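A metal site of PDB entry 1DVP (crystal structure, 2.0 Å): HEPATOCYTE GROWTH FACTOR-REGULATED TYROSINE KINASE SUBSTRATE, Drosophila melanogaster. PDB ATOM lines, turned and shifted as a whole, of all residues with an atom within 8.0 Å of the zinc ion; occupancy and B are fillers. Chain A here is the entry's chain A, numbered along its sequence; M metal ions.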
ATOM      1  N   VAL A 163      12.136  -6.419 -27.827  1.00  0.00           N
ATOM      2  CA  VAL A 163      12.736  -5.335 -28.557  1.00  0.00           C
ATOM      3  C   VAL A 163      12.896  -4.159 -27.630  1.00  0.00           C
ATOM      4  O   VAL A 163      12.184  -4.034 -26.619  1.00  0.00           O
ATOM      5  CB  VAL A 163      11.939  -4.936 -29.856  1.00  0.00           C
ATOM      6  CG1 VAL A 163      11.791  -6.152 -30.719  1.00  0.00           C
ATOM      7  CG2 VAL A 163      10.569  -4.273 -29.547  1.00  0.00           C
ATOM      8  N   CYS A 164      13.866  -3.303 -27.925  1.00  0.00           N
ATOM      9  CA  CYS A 164      14.062  -2.105 -27.090  1.00  0.00           C
ATOM     10  C   CYS A 164      12.832  -1.182 -27.184  1.00  0.00           C
ATOM     11  O   CYS A 164      12.499  -0.804 -28.273  1.00  0.00           O
ATOM     12  CB  CYS A 164      15.246  -1.287 -27.561  1.00  0.00           C
ATOM     13  SG  CYS A 164      15.176   0.399 -26.882  1.00  0.00           S
ATOM     14  N   HIS A 165      12.211  -0.784 -26.049  1.00  0.00           N
ATOM     15  CA  HIS A 165      10.985   0.027 -26.066  1.00  0.00           C
ATOM     16  C   HIS A 165      11.089   1.304 -26.935  1.00  0.00           C
ATOM     17  O   HIS A 165      10.131   1.692 -27.615  1.00  0.00           O
ATOM     18  CB  HIS A 165      10.638   0.435 -24.628  1.00  0.00           C
ATOM     19  CG  HIS A 165       9.302   1.110 -24.477  1.00  0.00           C
ATOM     20  ND1 HIS A 165       8.107   0.466 -24.724  1.00  0.00           N
ATOM     21  CD2 HIS A 165       8.976   2.367 -24.080  1.00  0.00           C
ATOM     22  CE1 HIS A 165       7.103   1.286 -24.498  1.00  0.00           C
ATOM     23  NE2 HIS A 165       7.602   2.447 -24.108  1.00  0.00           N
ATOM     24  N   ARG A 166      12.240   1.946 -26.904  1.00  0.00           N
ATOM     25  CA  ARG A 166      12.391   3.164 -27.645  1.00  0.00           C
ATOM     26  C   ARG A 166      12.718   3.022 -29.123  1.00  0.00           C
ATOM     27  O   ARG A 166      11.953   3.488 -29.994  1.00  0.00           O
ATOM     28  CB  ARG A 166      13.436   4.103 -26.959  1.00  0.00           C
ATOM     29  CG  ARG A 166      13.491   5.551 -27.552  1.00  0.00           C
ATOM     30  CD  ARG A 166      14.536   6.402 -26.816  1.00  0.00           C
ATOM     31  NE  ARG A 166      14.581   7.852 -27.149  1.00  0.00           N
ATOM     32  CZ  ARG A 166      13.697   8.779 -26.732  1.00  0.00           C
ATOM     33  NH1 ARG A 166      12.632   8.463 -25.990  1.00  0.00           N
ATOM     34  NH2 ARG A 166      13.935  10.056 -26.987  1.00  0.00           N
ATOM     35  N   CYS A 167      13.834   2.354 -29.420  1.00  0.00           N
ATOM     36  CA  CYS A 167      14.248   2.281 -30.826  1.00  0.00           C
ATOM     37  C   CYS A 167      13.778   1.043 -31.565  1.00  0.00           C
ATOM     38  O   CYS A 167      13.862   0.988 -32.786  1.00  0.00           O
ATOM     39  CB  CYS A 167      15.765   2.407 -30.902  1.00  0.00           C
ATOM     40  SG  CYS A 167      16.708   0.898 -30.448  1.00  0.00           S
ATOM     41  N   ARG A 168      13.253   0.069 -30.827  1.00  0.00           N
ATOM     42  CA  ARG A 168      12.758  -1.188 -31.346  1.00  0.00           C
ATOM     43  C   ARG A 168      13.829  -2.153 -31.828  1.00  0.00           C
ATOM     44  O   ARG A 168      13.526  -3.160 -32.452  1.00  0.00           O
ATOM     45  CB  ARG A 168      11.732  -0.977 -32.487  1.00  0.00           C
ATOM     46  CG  ARG A 168      10.672   0.105 -32.191  1.00  0.00           C
ATOM     47  CD  ARG A 168       9.939  -0.120 -30.846  1.00  0.00           C
ATOM     48  NE  ARG A 168       9.038  -1.252 -30.871  1.00  0.00           N
ATOM     49  CZ  ARG A 168       8.320  -1.638 -29.815  1.00  0.00           C
ATOM     50  NH1 ARG A 168       8.417  -0.965 -28.670  1.00  0.00           N
ATOM     51  NH2 ARG A 168       7.509  -2.687 -29.889  1.00  0.00           N
ATOM     52  N   VAL A 169      15.094  -1.910 -31.527  1.00  0.00           N
ATOM     53  CA  VAL A 169      16.100  -2.883 -32.000  1.00  0.00           C
ATOM     54  C   VAL A 169      15.819  -4.252 -31.296  1.00  0.00           C
ATOM     55  O   VAL A 169      15.403  -4.283 -30.114  1.00  0.00           O
ATOM     56  CB  VAL A 169      17.537  -2.384 -31.649  1.00  0.00           C
ATOM     57  CG1 VAL A 169      17.674  -2.319 -30.132  1.00  0.00           C
ATOM     58  CG2 VAL A 169      18.596  -3.245 -32.295  1.00  0.00           C
ATOM     59  N   GLU A 170      16.076  -5.354 -31.976  1.00  0.00           N
ATOM     60  CA  GLU A 170      15.808  -6.666 -31.369  1.00  0.00           C
ATOM     61  C   GLU A 170      16.951  -7.048 -30.463  1.00  0.00           C
ATOM     62  O   GLU A 170      18.120  -6.983 -30.867  1.00  0.00           O
ATOM     63  CB  GLU A 170      15.628  -7.758 -32.435  1.00  0.00           C
ATOM     64  CG  GLU A 170      14.463  -7.558 -33.317  1.00  0.00           C
ATOM     65  CD  GLU A 170      14.242  -8.718 -34.292  1.00  0.00           C
ATOM     66  OE1 GLU A 170      15.176  -9.428 -34.678  1.00  0.00           O
ATOM     67  OE2 GLU A 170      13.087  -8.912 -34.710  1.00  0.00           O
ATOM     68  N   PHE A 171      16.610  -7.446 -29.217  1.00  0.00           N
ATOM     69  CA  PHE A 171      17.662  -7.825 -28.303  1.00  0.00           C
ATOM     70  C   PHE A 171      18.289  -9.106 -28.807  1.00  0.00           C
ATOM     71  O   PHE A 171      17.619  -9.922 -29.375  1.00  0.00           O
ATOM     72  CB  PHE A 171      17.101  -8.088 -26.879  1.00  0.00           C
ATOM     73  CG  PHE A 171      16.574  -6.842 -26.192  1.00  0.00           C
ATOM     74  CD1 PHE A 171      15.267  -6.789 -25.737  1.00  0.00           C
ATOM     75  CD2 PHE A 171      17.401  -5.725 -26.025  1.00  0.00           C
ATOM     76  CE1 PHE A 171      14.763  -5.681 -25.144  1.00  0.00           C
ATOM     77  CE2 PHE A 171      16.922  -4.594 -25.433  1.00  0.00           C
ATOM     78  CZ  PHE A 171      15.593  -4.540 -24.981  1.00  0.00           C
ATOM     79  N   ASN A 175      23.421  -7.862 -27.354  1.00  0.00           N
ATOM     80  CA  ASN A 175      22.754  -6.554 -27.266  1.00  0.00           C
ATOM     81  C   ASN A 175      21.547  -6.828 -26.378  1.00  0.00           C
ATOM     82  O   ASN A 175      20.443  -6.901 -26.842  1.00  0.00           O
ATOM     83  CB  ASN A 175      22.343  -6.105 -28.683  1.00  0.00           C
ATOM     84  CG  ASN A 175      21.955  -4.638 -28.774  1.00  0.00           C
ATOM     85  OD1 ASN A 175      21.871  -3.940 -27.785  1.00  0.00           O
ATOM     86  ND2 ASN A 175      21.709  -4.160 -30.013  1.00  0.00           N
ATOM     87  N   VAL A 186      12.066  -1.952 -20.770  1.00  0.00           N
ATOM     88  CA  VAL A 186      13.359  -2.550 -21.137  1.00  0.00           C
ATOM     89  C   VAL A 186      13.752  -1.803 -22.400  1.00  0.00           C
ATOM     90  O   VAL A 186      12.872  -1.480 -23.199  1.00  0.00           O
ATOM     91  CB  VAL A 186      13.329  -4.090 -21.470  1.00  0.00           C
ATOM     92  CG1 VAL A 186      13.208  -4.914 -20.155  1.00  0.00           C
ATOM     93  CG2 VAL A 186      12.170  -4.397 -22.356  1.00  0.00           C
ATOM     94  N   PHE A 187      15.057  -1.544 -22.505  1.00  0.00           N
ATOM     95  CA  PHE A 187      15.711  -0.815 -23.588  1.00  0.00           C
ATOM     96  C   PHE A 187      17.101  -1.405 -23.824  1.00  0.00           C
ATOM     97  O   PHE A 187      17.650  -2.155 -22.964  1.00  0.00           O
ATOM     98  CB  PHE A 187      15.947   0.659 -23.178  1.00  0.00           C
ATOM     99  CG  PHE A 187      14.698   1.392 -22.718  1.00  0.00           C
ATOM    100  CD1 PHE A 187      14.166   1.222 -21.423  1.00  0.00           C
ATOM    101  CD2 PHE A 187      14.056   2.289 -23.576  1.00  0.00           C
ATOM    102  CE1 PHE A 187      13.023   1.930 -20.995  1.00  0.00           C
ATOM    103  CE2 PHE A 187      12.935   2.990 -23.178  1.00  0.00           C
ATOM    104  CZ  PHE A 187      12.403   2.804 -21.856  1.00  0.00           C
ATOM    105  N   CYS A 188      17.662  -1.058 -24.987  1.00  0.00           N
ATOM    106  CA  CYS A 188      19.015  -1.452 -25.345  1.00  0.00           C
ATOM    107  C   CYS A 188      19.933  -0.474 -24.522  1.00  0.00           C
ATOM    108  O   CYS A 188      19.476   0.489 -23.928  1.00  0.00           O
ATOM    109  CB  CYS A 188      19.277  -1.254 -26.840  1.00  0.00           C
ATOM    110  SG  CYS A 188      19.203   0.482 -27.379  1.00  0.00           S
ATOM    111  N   GLY A 189      21.201  -0.807 -24.461  1.00  0.00           N
ATOM    112  CA  GLY A 189      22.168  -0.014 -23.719  1.00  0.00           C
ATOM    113  C   GLY A 189      22.308   1.395 -24.320  1.00  0.00           C
ATOM    114  O   GLY A 189      22.422   2.348 -23.560  1.00  0.00           O
ATOM    115  N   GLN A 190      22.269   1.550 -25.652  1.00  0.00           N
ATOM    116  CA  GLN A 190      22.376   2.884 -26.224  1.00  0.00           C
ATOM    117  C   GLN A 190      21.169   3.753 -25.974  1.00  0.00           C
ATOM    118  O   GLN A 190      21.299   4.935 -26.040  1.00  0.00           O
ATOM    119  CB  GLN A 190      22.661   2.876 -27.748  1.00  0.00           C
ATOM    120  CG  GLN A 190      23.818   2.028 -28.053  1.00  0.00           C
ATOM    121  CD  GLN A 190      23.949   1.819 -29.525  1.00  0.00           C
ATOM    122  OE1 GLN A 190      24.418   2.697 -30.243  1.00  0.00           O
ATOM    123  NE2 GLN A 190      23.459   0.688 -30.000  1.00  0.00           N
ATOM    124  N   CYS A 191      19.988   3.183 -25.690  1.00  0.00           N
ATOM    125  CA  CYS A 191      18.872   4.061 -25.329  1.00  0.00           C
ATOM    126  C   CYS A 191      18.780   4.333 -23.804  1.00  0.00           C
ATOM    127  O   CYS A 191      17.886   5.032 -23.384  1.00  0.00           O
ATOM    128  CB  CYS A 191      17.530   3.482 -25.801  1.00  0.00           C
ATOM    129  SG  CYS A 191      17.300   3.603 -27.639  1.00  0.00           S
ATOM    130  N   THR A 192      19.693   3.771 -23.019  1.00  0.00           N
ATOM    131  CA  THR A 192      19.731   3.946 -21.551  1.00  0.00           C
ATOM    132  C   THR A 192      21.192   4.138 -21.109  1.00  0.00           C
ATOM    133  O   THR A 192      21.648   3.527 -20.144  1.00  0.00           O
ATOM    134  CB  THR A 192      19.134   2.668 -20.787  1.00  0.00           C
ATOM    135  OG1 THR A 192      19.652   1.450 -21.354  1.00  0.00           O
ATOM    136  CG2 THR A 192      17.667   2.679 -20.908  1.00  0.00           C
ATOM    137  N   ASP A 211      16.147   7.501 -22.503  1.00  0.00           N
ATOM    138  CA  ASP A 211      16.195   8.841 -23.072  1.00  0.00           C
ATOM    139  C   ASP A 211      14.916   9.605 -22.849  1.00  0.00           C
ATOM    140  O   ASP A 211      14.975  10.722 -22.441  1.00  0.00           O
ATOM    141  CB  ASP A 211      16.564   8.742 -24.565  1.00  0.00           C
ATOM    142  CG  ASP A 211      18.021   8.414 -24.734  1.00  0.00           C
ATOM    143  OD1 ASP A 211      18.752   8.639 -23.776  1.00  0.00           O
ATOM    144  OD2 ASP A 211      18.466   7.934 -25.791  1.00  0.00           O
HETATM  145 ZN    ZN M   1      17.234   1.260 -28.047  1.00  0.00          ZN
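The side-chain hydroxyl of Thr 192 lies within hydrogen-bond range of the backbone carbonyl oxygen of Cys 188, at 2.8 Å. The backbone carbonyl oxygen (O) of Cys 191 sits at hydrogen-bond distance from the backbone NH (N) of Asp 211. The side-chain sulfur (SG) of Cys 188 lies close to the backbone NH (N) of Gln 190, at 3.7 Å. The side-chain sulfur (SG) of Cys 167 lies close to the backbone NH (N) of Val 169 (3.4 Å). N of Cys 164 is in hydrogen-bond range of O of Val 169 (2.8 Å). N of Arg 166 lies close to SG of Cys 164 (3.3 Å).
Four residues have an atom within 4 Å of the zinc ion: Cys 164, Cys 167, Cys 188 and Cys 191.
The zinc ion is bound by SG of Cys 188 (2.2 Å), SG of Cys 191 (2.4 Å), SG of Cys 167 (2.5 Å) and SG of Cys 164 (2.5 Å).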
